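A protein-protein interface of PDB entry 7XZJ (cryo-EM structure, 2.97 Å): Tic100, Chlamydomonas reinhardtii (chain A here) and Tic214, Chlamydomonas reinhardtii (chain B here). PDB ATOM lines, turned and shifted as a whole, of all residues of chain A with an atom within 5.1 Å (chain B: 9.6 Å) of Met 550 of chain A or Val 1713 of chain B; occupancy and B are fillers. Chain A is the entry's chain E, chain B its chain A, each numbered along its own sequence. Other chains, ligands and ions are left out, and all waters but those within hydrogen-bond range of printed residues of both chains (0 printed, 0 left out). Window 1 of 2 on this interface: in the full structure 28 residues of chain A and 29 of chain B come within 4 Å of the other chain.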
ATOM      1  N   MET A 542      -8.280 -12.652  26.261  1.00  0.00           N
ATOM      2  CA  MET A 542      -9.263 -11.879  27.067  1.00  0.00           C
ATOM      3  C   MET A 542     -10.448 -11.480  26.181  1.00  0.00           C
ATOM      4  O   MET A 542     -10.223 -11.176  24.993  1.00  0.00           O
ATOM      5  CB  MET A 542      -8.622 -10.621  27.662  1.00  0.00           C
ATOM      6  CG  MET A 542      -8.115  -9.640  26.623  1.00  0.00           C
ATOM      7  SD  MET A 542      -7.220  -8.260  27.379  1.00  0.00           S
ATOM      8  CE  MET A 542      -8.423  -7.712  28.589  1.00  0.00           C
ATOM      9  N   ILE A 546     -14.350  -6.774  26.860  1.00  0.00           N
ATOM     10  CA  ILE A 546     -13.647  -6.372  28.115  1.00  0.00           C
ATOM     11  C   ILE A 546     -12.364  -5.628  27.736  1.00  0.00           C
ATOM     12  O   ILE A 546     -12.062  -4.605  28.375  1.00  0.00           O
ATOM     13  CB  ILE A 546     -13.368  -7.601  29.005  1.00  0.00           C
ATOM     14  CG1 ILE A 546     -14.666  -8.284  29.442  1.00  0.00           C
ATOM     15  CG2 ILE A 546     -12.504  -7.230  30.201  1.00  0.00           C
ATOM     16  CD1 ILE A 546     -15.587  -7.395  30.243  1.00  0.00           C
ATOM     17  N   ARG A 547     -11.655  -6.114  26.714  1.00  0.00           N
ATOM     18  CA  ARG A 547     -10.377  -5.482  26.298  1.00  0.00           C
ATOM     19  C   ARG A 547     -10.646  -4.048  25.835  1.00  0.00           C
ATOM     20  O   ARG A 547      -9.871  -3.152  26.216  1.00  0.00           O
ATOM     21  CB  ARG A 547      -9.740  -6.306  25.176  1.00  0.00           C
ATOM     22  CG  ARG A 547      -8.396  -5.779  24.694  1.00  0.00           C
ATOM     23  CD  ARG A 547      -7.722  -6.686  23.681  1.00  0.00           C
ATOM     24  NE  ARG A 547      -8.470  -6.827  22.440  1.00  0.00           N
ATOM     25  CZ  ARG A 547      -9.155  -7.909  22.086  1.00  0.00           C
ATOM     26  NH1 ARG A 547      -9.183  -8.965  22.881  1.00  0.00           N
ATOM     27  NH2 ARG A 547      -9.802  -7.933  20.936  1.00  0.00           N
ATOM     28  N   GLU A 548     -11.716  -3.842  25.061  1.00  0.00           N
ATOM     29  CA  GLU A 548     -12.056  -2.484  24.557  1.00  0.00           C
ATOM     30  C   GLU A 548     -12.389  -1.570  25.739  1.00  0.00           C
ATOM     31  O   GLU A 548     -11.954  -0.403  25.719  1.00  0.00           O
ATOM     32  CB  GLU A 548     -13.221  -2.552  23.569  1.00  0.00           C
ATOM     33  CG  GLU A 548     -12.898  -3.323  22.305  1.00  0.00           C
ATOM     34  CD  GLU A 548     -11.767  -2.754  21.465  1.00  0.00           C
ATOM     35  OE1 GLU A 548     -11.665  -1.516  21.369  1.00  0.00           O
ATOM     36  OE2 GLU A 548     -10.987  -3.555  20.912  1.00  0.00           O
ATOM     37  N   LEU A 549     -13.128  -2.086  26.724  1.00  0.00           N
ATOM     38  CA  LEU A 549     -13.515  -1.275  27.908  1.00  0.00           C
ATOM     39  C   LEU A 549     -12.252  -0.866  28.672  1.00  0.00           C
ATOM     40  O   LEU A 549     -12.090   0.338  28.933  1.00  0.00           O
ATOM     41  CB  LEU A 549     -14.442  -2.112  28.793  1.00  0.00           C
ATOM     42  CG  LEU A 549     -14.913  -1.438  30.080  1.00  0.00           C
ATOM     43  CD1 LEU A 549     -15.763  -0.215  29.770  1.00  0.00           C
ATOM     44  CD2 LEU A 549     -15.687  -2.417  30.949  1.00  0.00           C
ATOM     45  N   MET A 550     -11.396  -1.832  29.012  1.00  0.00           N
ATOM     46  CA  MET A 550     -10.193  -1.535  29.780  1.00  0.00           C
ATOM     47  C   MET A 550      -9.294  -0.547  29.049  1.00  0.00           C
ATOM     48  O   MET A 550      -8.697   0.332  29.673  1.00  0.00           O
ATOM     49  CB  MET A 550      -9.437  -2.825  30.094  1.00  0.00           C
ATOM     50  CG  MET A 550     -10.173  -3.734  31.062  1.00  0.00           C
ATOM     51  SD  MET A 550      -9.136  -5.067  31.686  1.00  0.00           S
ATOM     52  CE  MET A 550      -7.891  -4.130  32.564  1.00  0.00           C
ATOM     53  N   ALA A 551      -9.177  -0.677  27.726  1.00  0.00           N
ATOM     54  CA  ALA A 551      -8.382   0.280  26.959  1.00  0.00           C
ATOM     55  C   ALA A 551      -8.980   1.679  27.045  1.00  0.00           C
ATOM     56  O   ALA A 551      -8.260   2.670  27.232  1.00  0.00           O
ATOM     57  CB  ALA A 551      -8.277  -0.175  25.505  1.00  0.00           C
ATOM     58  N   ALA A 552     -10.305   1.765  26.915  1.00  0.00           N
ATOM     59  CA  ALA A 552     -10.985   3.079  26.994  1.00  0.00           C
ATOM     60  C   ALA A 552     -10.707   3.712  28.360  1.00  0.00           C
ATOM     61  O   ALA A 552     -10.358   4.919  28.412  1.00  0.00           O
ATOM     62  CB  ALA A 552     -12.464   2.903  26.763  1.00  0.00           C
ATOM     63  N   GLU A 553     -10.864   2.926  29.429  1.00  0.00           N
ATOM     64  CA  GLU A 553     -10.589   3.453  30.761  1.00  0.00           C
ATOM     65  C   GLU A 553      -9.124   3.849  30.906  1.00  0.00           C
ATOM     66  O   GLU A 553      -8.802   4.863  31.538  1.00  0.00           O
ATOM     67  CB  GLU A 553     -10.982   2.423  31.816  1.00  0.00           C
ATOM     68  CG  GLU A 553     -12.469   2.136  31.857  1.00  0.00           C
ATOM     69  CD  GLU A 553     -13.293   3.376  32.115  1.00  0.00           C
ATOM     70  OE1 GLU A 553     -12.873   4.208  32.948  1.00  0.00           O
ATOM     71  OE2 GLU A 553     -14.363   3.515  31.488  1.00  0.00           O
ATOM     72  N   GLY A 554      -8.222   3.060  30.325  1.00  0.00           N
ATOM     73  CA  GLY A 554      -6.808   3.377  30.405  1.00  0.00           C
ATOM     74  C   GLY A 554      -6.456   4.675  29.711  1.00  0.00           C
ATOM     75  O   GLY A 554      -5.502   5.355  30.097  1.00  0.00           O
ATOM     76  N   MET A 555      -7.260   5.043  28.708  1.00  0.00           N
ATOM     77  CA  MET A 555      -7.051   6.341  28.013  1.00  0.00           C
ATOM     78  C   MET A 555      -7.587   7.449  28.921  1.00  0.00           C
ATOM     79  O   MET A 555      -6.962   8.525  28.979  1.00  0.00           O
ATOM     80  CB  MET A 555      -7.810   6.379  26.684  1.00  0.00           C
ATOM     81  CG  MET A 555      -7.504   5.205  25.777  1.00  0.00           C
ATOM     82  SD  MET A 555      -8.481   5.229  24.253  1.00  0.00           S
ATOM     83  CE  MET A 555      -7.834   6.705  23.470  1.00  0.00           C
ATOM     84  N   ASN B1071     -17.978   0.240  22.433  1.00  0.00           N
ATOM     85  CA  ASN B1071     -16.804   0.590  23.276  1.00  0.00           C
ATOM     86  C   ASN B1071     -15.684   1.107  22.369  1.00  0.00           C
ATOM     87  O   ASN B1071     -15.023   2.093  22.750  1.00  0.00           O
ATOM     88  CB  ASN B1071     -16.327  -0.602  24.107  1.00  0.00           C
ATOM     89  CG  ASN B1071     -17.372  -1.115  25.076  1.00  0.00           C
ATOM     90  OD1 ASN B1071     -18.425  -0.505  25.242  1.00  0.00           O
ATOM     91  ND2 ASN B1071     -17.087  -2.234  25.720  1.00  0.00           N
ATOM     92  N   TYR B1072     -15.487   0.461  21.217  1.00  0.00           N
ATOM     93  CA  TYR B1072     -14.390   0.859  20.297  1.00  0.00           C
ATOM     94  C   TYR B1072     -14.613   2.279  19.767  1.00  0.00           C
ATOM     95  O   TYR B1072     -13.643   3.053  19.759  1.00  0.00           O
ATOM     96  CB  TYR B1072     -14.264  -0.139  19.142  1.00  0.00           C
ATOM     97  CG  TYR B1072     -13.522   0.384  17.937  1.00  0.00           C
ATOM     98  CD1 TYR B1072     -12.140   0.478  17.933  1.00  0.00           C
ATOM     99  CD2 TYR B1072     -14.201   0.788  16.800  1.00  0.00           C
ATOM    100  CE1 TYR B1072     -11.452   0.963  16.834  1.00  0.00           C
ATOM    101  CE2 TYR B1072     -13.528   1.278  15.692  1.00  0.00           C
ATOM    102  CZ  TYR B1072     -12.149   1.362  15.707  1.00  0.00           C
ATOM    103  OH  TYR B1072     -11.479   1.839  14.617  1.00  0.00           O
ATOM    104  N   HIS B1075     -13.873   5.226  22.454  1.00  0.00           N
ATOM    105  CA  HIS B1075     -12.422   5.512  22.605  1.00  0.00           C
ATOM    106  C   HIS B1075     -11.843   6.064  21.299  1.00  0.00           C
ATOM    107  O   HIS B1075     -11.012   6.987  21.370  1.00  0.00           O
ATOM    108  CB  HIS B1075     -11.678   4.307  23.204  1.00  0.00           C
ATOM    109  CG  HIS B1075     -11.003   3.410  22.220  1.00  0.00           C
ATOM    110  ND1 HIS B1075     -11.518   2.177  21.876  1.00  0.00           N
ATOM    111  CD2 HIS B1075      -9.847   3.540  21.535  1.00  0.00           C
ATOM    112  CE1 HIS B1075     -10.718   1.596  21.006  1.00  0.00           C
ATOM    113  NE2 HIS B1075      -9.686   2.413  20.779  1.00  0.00           N
ATOM    114  N   LYS B1079     -12.677  10.068  22.751  1.00  0.00           N
ATOM    115  CA  LYS B1079     -11.467  10.255  23.592  1.00  0.00           C
ATOM    116  C   LYS B1079     -10.424  11.081  22.832  1.00  0.00           C
ATOM    117  O   LYS B1079      -9.805  11.962  23.455  1.00  0.00           O
ATOM    118  CB  LYS B1079     -10.926   8.910  24.084  1.00  0.00           C
ATOM    119  CG  LYS B1079     -11.839   8.160  25.044  1.00  0.00           C
ATOM    120  CD  LYS B1079     -12.180   8.948  26.290  1.00  0.00           C
ATOM    121  CE  LYS B1079     -10.977   9.240  27.160  1.00  0.00           C
ATOM    122  NZ  LYS B1079     -11.333  10.096  28.315  1.00  0.00           N
ATOM    123  N   ASN B1705      -0.363  -3.756  16.125  1.00  0.00           N
ATOM    124  CA  ASN B1705      -1.501  -3.065  16.742  1.00  0.00           C
ATOM    125  C   ASN B1705      -1.935  -3.751  18.039  1.00  0.00           C
ATOM    126  O   ASN B1705      -2.353  -3.084  19.005  1.00  0.00           O
ATOM    127  CB  ASN B1705      -2.671  -2.955  15.761  1.00  0.00           C
ATOM    128  CG  ASN B1705      -3.132  -4.296  15.243  1.00  0.00           C
ATOM    129  OD1 ASN B1705      -3.692  -5.102  15.984  1.00  0.00           O
ATOM    130  ND2 ASN B1705      -2.927  -4.530  13.954  1.00  0.00           N
ATOM    131  N   GLN B1706      -1.840  -5.082  18.082  1.00  0.00           N
ATOM    132  CA  GLN B1706      -2.275  -5.810  19.266  1.00  0.00           C
ATOM    133  C   GLN B1706      -1.459  -5.415  20.489  1.00  0.00           C
ATOM    134  O   GLN B1706      -2.003  -5.292  21.594  1.00  0.00           O
ATOM    135  CB  GLN B1706      -2.182  -7.314  19.022  1.00  0.00           C
ATOM    136  CG  GLN B1706      -3.159  -7.824  17.981  1.00  0.00           C
ATOM    137  CD  GLN B1706      -2.988  -9.303  17.715  1.00  0.00           C
ATOM    138  OE1 GLN B1706      -1.911  -9.864  17.921  1.00  0.00           O
ATOM    139  NE2 GLN B1706      -4.054  -9.947  17.252  1.00  0.00           N
ATOM    140  N   ILE B1707      -0.151  -5.218  20.317  1.00  0.00           N
ATOM    141  CA  ILE B1707       0.684  -4.858  21.461  1.00  0.00           C
ATOM    142  C   ILE B1707       0.286  -3.493  22.009  1.00  0.00           C
ATOM    143  O   ILE B1707       0.320  -3.269  23.222  1.00  0.00           O
ATOM    144  CB  ILE B1707       2.181  -4.912  21.097  1.00  0.00           C
ATOM    145  CG1 ILE B1707       2.514  -3.912  19.991  1.00  0.00           C
ATOM    146  CG2 ILE B1707       2.583  -6.326  20.713  1.00  0.00           C
ATOM    147  CD1 ILE B1707       3.968  -3.892  19.596  1.00  0.00           C
ATOM    148  N   LYS B1708      -0.095  -2.557  21.135  1.00  0.00           N
ATOM    149  CA  LYS B1708      -0.558  -1.255  21.611  1.00  0.00           C
ATOM    150  C   LYS B1708      -1.835  -1.394  22.429  1.00  0.00           C
ATOM    151  O   LYS B1708      -1.985  -0.765  23.490  1.00  0.00           O
ATOM    152  CB  LYS B1708      -0.785  -0.315  20.429  1.00  0.00           C
ATOM    153  CG  LYS B1708      -1.291   1.060  20.821  1.00  0.00           C
ATOM    154  CD  LYS B1708      -0.325   1.762  21.758  1.00  0.00           C
ATOM    155  CE  LYS B1708      -0.606   3.253  21.816  1.00  0.00           C
ATOM    156  NZ  LYS B1708      -1.985   3.545  22.302  1.00  0.00           N
ATOM    157  N   THR B1709      -2.770  -2.216  21.950  1.00  0.00           N
ATOM    158  CA  THR B1709      -3.988  -2.436  22.729  1.00  0.00           C
ATOM    159  C   THR B1709      -3.663  -3.048  24.091  1.00  0.00           C
ATOM    160  O   THR B1709      -4.232  -2.653  25.123  1.00  0.00           O
ATOM    161  CB  THR B1709      -4.959  -3.327  21.959  1.00  0.00           C
ATOM    162  OG1 THR B1709      -5.141  -2.802  20.640  1.00  0.00           O
ATOM    163  CG2 THR B1709      -6.308  -3.360  22.664  1.00  0.00           C
ATOM    164  N   LYS B1710      -2.735  -4.007  24.115  1.00  0.00           N
ATOM    165  CA  LYS B1710      -2.327  -4.612  25.377  1.00  0.00           C
ATOM    166  C   LYS B1710      -1.668  -3.589  26.295  1.00  0.00           C
ATOM    167  O   LYS B1710      -1.832  -3.645  27.518  1.00  0.00           O
ATOM    168  CB  LYS B1710      -1.377  -5.778  25.117  1.00  0.00           C
ATOM    169  CG  LYS B1710      -0.871  -6.466  26.373  1.00  0.00           C
ATOM    170  CD  LYS B1710      -2.008  -7.080  27.168  1.00  0.00           C
ATOM    171  CE  LYS B1710      -1.479  -7.909  28.326  1.00  0.00           C
ATOM    172  NZ  LYS B1710      -2.571  -8.342  29.242  1.00  0.00           N
ATOM    173  N   LYS B1711      -0.897  -2.661  25.724  1.00  0.00           N
ATOM    174  CA  LYS B1711      -0.281  -1.608  26.524  1.00  0.00           C
ATOM    175  C   LYS B1711      -1.336  -0.742  27.194  1.00  0.00           C
ATOM    176  O   LYS B1711      -1.198  -0.375  28.368  1.00  0.00           O
ATOM    177  CB  LYS B1711       0.626  -0.744  25.650  1.00  0.00           C
ATOM    178  CG  LYS B1711       1.851  -1.455  25.120  1.00  0.00           C
ATOM    179  CD  LYS B1711       2.674  -0.523  24.247  1.00  0.00           C
ATOM    180  CE  LYS B1711       3.923  -1.213  23.724  1.00  0.00           C
ATOM    181  NZ  LYS B1711       4.725  -0.317  22.846  1.00  0.00           N
ATOM    182  N   LEU B1712      -2.391  -0.388  26.457  1.00  0.00           N
ATOM    183  CA  LEU B1712      -3.469   0.390  27.067  1.00  0.00           C
ATOM    184  C   LEU B1712      -4.142  -0.386  28.195  1.00  0.00           C
ATOM    185  O   LEU B1712      -4.435   0.173  29.264  1.00  0.00           O
ATOM    186  CB  LEU B1712      -4.494   0.796  26.010  1.00  0.00           C
ATOM    187  CG  LEU B1712      -4.449   2.265  25.592  1.00  0.00           C
ATOM    188  CD1 LEU B1712      -3.063   2.636  25.092  1.00  0.00           C
ATOM    189  CD2 LEU B1712      -5.503   2.564  24.535  1.00  0.00           C
ATOM    190  N   VAL B1713      -4.384  -1.683  27.981  1.00  0.00           N
ATOM    191  CA  VAL B1713      -4.982  -2.499  29.039  1.00  0.00           C
ATOM    192  C   VAL B1713      -4.079  -2.526  30.268  1.00  0.00           C
ATOM    193  O   VAL B1713      -4.548  -2.418  31.412  1.00  0.00           O
ATOM    194  CB  VAL B1713      -5.276  -3.918  28.520  1.00  0.00           C
ATOM    195  CG1 VAL B1713      -5.659  -4.829  29.669  1.00  0.00           C
ATOM    196  CG2 VAL B1713      -6.386  -3.876  27.487  1.00  0.00           C
ATOM    197  N   ALA B1714      -2.773  -2.686  30.050  1.00  0.00           N
ATOM    198  CA  ALA B1714      -1.821  -2.718  31.154  1.00  0.00           C
ATOM    199  C   ALA B1714      -1.817  -1.402  31.916  1.00  0.00           C
ATOM    200  O   ALA B1714      -1.760  -1.386  33.153  1.00  0.00           O
ATOM    201  CB  ALA B1714      -0.423  -3.039  30.628  1.00  0.00           C
ATOM    202  N   ARG B1715      -1.877  -0.282  31.194  1.00  0.00           N
ATOM    203  CA  ARG B1715      -1.933   1.008  31.868  1.00  0.00           C
ATOM    204  C   ARG B1715      -3.180   1.111  32.729  1.00  0.00           C
ATOM    205  O   ARG B1715      -3.119   1.602  33.861  1.00  0.00           O
ATOM    206  CB  ARG B1715      -1.892   2.147  30.849  1.00  0.00           C
ATOM    207  CG  ARG B1715      -1.727   3.536  31.469  1.00  0.00           C
ATOM    208  CD  ARG B1715      -3.063   4.197  31.769  1.00  0.00           C
ATOM    209  NE  ARG B1715      -2.919   5.349  32.647  1.00  0.00           N
ATOM    210  N   ARG B1716      -4.305   0.606  32.229  1.00  0.00           N
ATOM    211  CA  ARG B1716      -5.575   0.731  32.989  1.00  0.00           C
ATOM    212  C   ARG B1716      -5.505  -0.127  34.254  1.00  0.00           C
ATOM    213  O   ARG B1716      -5.962   0.351  35.304  1.00  0.00           O
ATOM    214  CB  ARG B1716      -6.772   0.314  32.130  1.00  0.00           C
ATOM    215  CG  ARG B1716      -8.122   0.523  32.799  1.00  0.00           C
ATOM    216  CD  ARG B1716      -8.550  -0.659  33.646  1.00  0.00           C
ATOM    217  NE  ARG B1716      -9.744  -0.370  34.426  1.00  0.00           N
ATOM    218  CZ  ARG B1716      -9.732   0.075  35.675  1.00  0.00           C
ATOM    219  NH1 ARG B1716      -8.582   0.276  36.295  1.00  0.00           N
ATOM    220  NH2 ARG B1716     -10.870   0.311  36.304  1.00  0.00           N
ATOM    221  N   ILE B1717      -4.952  -1.340  34.181  1.00  0.00           N
ATOM    222  CA  ILE B1717      -4.976  -2.212  35.396  1.00  0.00           C
ATOM    223  C   ILE B1717      -3.890  -1.757  36.380  1.00  0.00           C
ATOM    224  O   ILE B1717      -4.242  -1.451  37.535  1.00  0.00           O
ATOM    225  CB  ILE B1717      -4.895  -3.716  35.048  1.00  0.00           C
ATOM    226  CG1 ILE B1717      -4.801  -4.590  36.301  1.00  0.00           C
ATOM    227  CG2 ILE B1717      -3.772  -4.020  34.069  1.00  0.00           C
ATOM    228  CD1 ILE B1717      -4.645  -6.063  36.009  1.00  0.00           C
ATOM    229  N   LYS B1718      -2.631  -1.705  35.943  1.00  0.00           N
ATOM    230  CA  LYS B1718      -1.508  -1.355  36.856  1.00  0.00           C
ATOM    231  C   LYS B1718      -1.611   0.085  37.372  1.00  0.00           C
ATOM    232  O   LYS B1718      -1.337   0.285  38.571  1.00  0.00           O
ATOM    233  CB  LYS B1718      -0.159  -1.590  36.168  1.00  0.00           C
ATOM    234  CG  LYS B1718       0.430  -2.987  36.323  1.00  0.00           C
ATOM    235  CD  LYS B1718      -0.327  -4.068  35.579  1.00  0.00           C
ATOM    236  CE  LYS B1718       0.318  -5.434  35.693  1.00  0.00           C
ATOM    237  NZ  LYS B1718      -0.476  -6.476  35.002  1.00  0.00           N
ATOM    238  N   LYS B1719      -1.989   1.049  36.525  1.00  0.00           N
ATOM    239  CA  LYS B1719      -1.953   2.472  36.973  1.00  0.00           C
ATOM    240  C   LYS B1719      -3.292   3.190  36.777  1.00  0.00           C
ATOM    241  O   LYS B1719      -3.345   4.088  35.914  1.00  0.00           O
ATOM    242  CB  LYS B1719      -0.839   3.228  36.244  1.00  0.00           C
ATOM    243  N   ARG B1720      -4.320   2.832  37.548  1.00  0.00           N
ATOM    244  CA  ARG B1720      -5.601   3.574  37.504  1.00  0.00           C
ATOM    245  C   ARG B1720      -5.398   4.847  38.315  1.00  0.00           C
ATOM    246  O   ARG B1720      -4.810   4.758  39.408  1.00  0.00           O
ATOM    247  CB  ARG B1720      -6.737   2.730  38.085  1.00  0.00           C
ATOM    248  CG  ARG B1720      -8.085   3.436  38.128  1.00  0.00           C
ATOM    249  CD  ARG B1720      -8.738   3.576  36.766  1.00  0.00           C
ATOM    250  NE  ARG B1720      -8.011   4.461  35.867  1.00  0.00           N
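The backbone carbonyl oxygen of Tyr 1072 of chain B sits at hydrogen-bond distance from a ring nitrogen (ND1) of His 1075 of chain B. The side-chain hydroxyl (OG1) of Thr 1709 of chain B lies within hydrogen-bond range of the backbone carbonyl oxygen (O) of Asn 1705 of chain B, at 3.2 Å. O of Met 542 of chain A is in hydrogen-bond range of NH1 of Arg 547 of chain A.
CB of Asn 1071 of chain B touches CB of Glu 548 of chain A, 3.7 Å away. CB of Tyr 1072 of chain B touches OE1 of Glu 548 of chain A (3.7 Å). Val 1713 of chain B touches Met 550 of chain A. Met 550 of chain A touches Arg 1716 of chain B (O to CB, 3.1 Å). Met 550 of chain A touches Ile 1717 of chain B. Glu 553 of chain A touches Arg 1716 of chain B (CB to CG, 3.6 Å). Arg 1715 of chain B touches Gly 554 of chain A. Gly 554 of chain A touches Arg 1716 of chain B. Met 555 of chain A touches His 1075 of chain B. Met 555 of chain A touches Leu 1712 of chain B.
Printed residues of chain B within 4 Å of Arg 547 of chain A: Thr 1709 (3.8 Å) and Val 1713 (3.8 Å). No residue of chain B comes within 4 Å of Leu 549 of chain A. Met 550 of chain A touches just these residues of chain B: Val 1713 (3.7 Å), Arg 1716 (3.1 Å) and Ile 1717 (3.9 Å). Of chain B, only Leu 1712 (3.9 Å) comes within 4 Å of Ala 551 of chain A. Ala 552 of chain A touches just one residue of chain B: His 1075 (3.9 Å). Printed residues of chain A within 4 Å of His 1075 of chain B: Glu 548, Ala 552 and Met 555. Of the printed residues of chain A, Lys 1079 of chain B touches Met 555. Lys 1710 of chain B touches none of the printed residues of chain A. Of the printed residues of chain A, Leu 1712 of chain B touches Ala 551 (3.9 Å) and Met 555 (3.5 Å). Of chain A, only Arg 547 (3.8 Å) and Met 550 (3.7 Å) come within 4 Å of Val 1713 of chain B. Of the printed residues of chain A, Arg 1716 of chain B touches Met 550 (3.1 Å), Glu 553 (3.6 Å) and Gly 554 (3.5 Å). Lys 1719 of chain B touches none of the printed residues of chain A. The nearest residue of chain B that does not touch Met 550 of chain A is Leu 1712 of chain B (4.3 Å). The nearest printed residue of chain B that does not touch Met 555 of chain A is Arg 1715 of chain B (5.3 Å).
Of the 11 printed residues of chain A, 8 touch a printed residue of chain B. Printed residues of chain A that touch a printed residue of chain B: Arg 547, Glu 548, Met 550, Ala 551, Ala 552, Glu 553, Gly 554 and Met 555. Along chain A the printed residues that touch a printed residue of chain B span positions 547 to 555.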
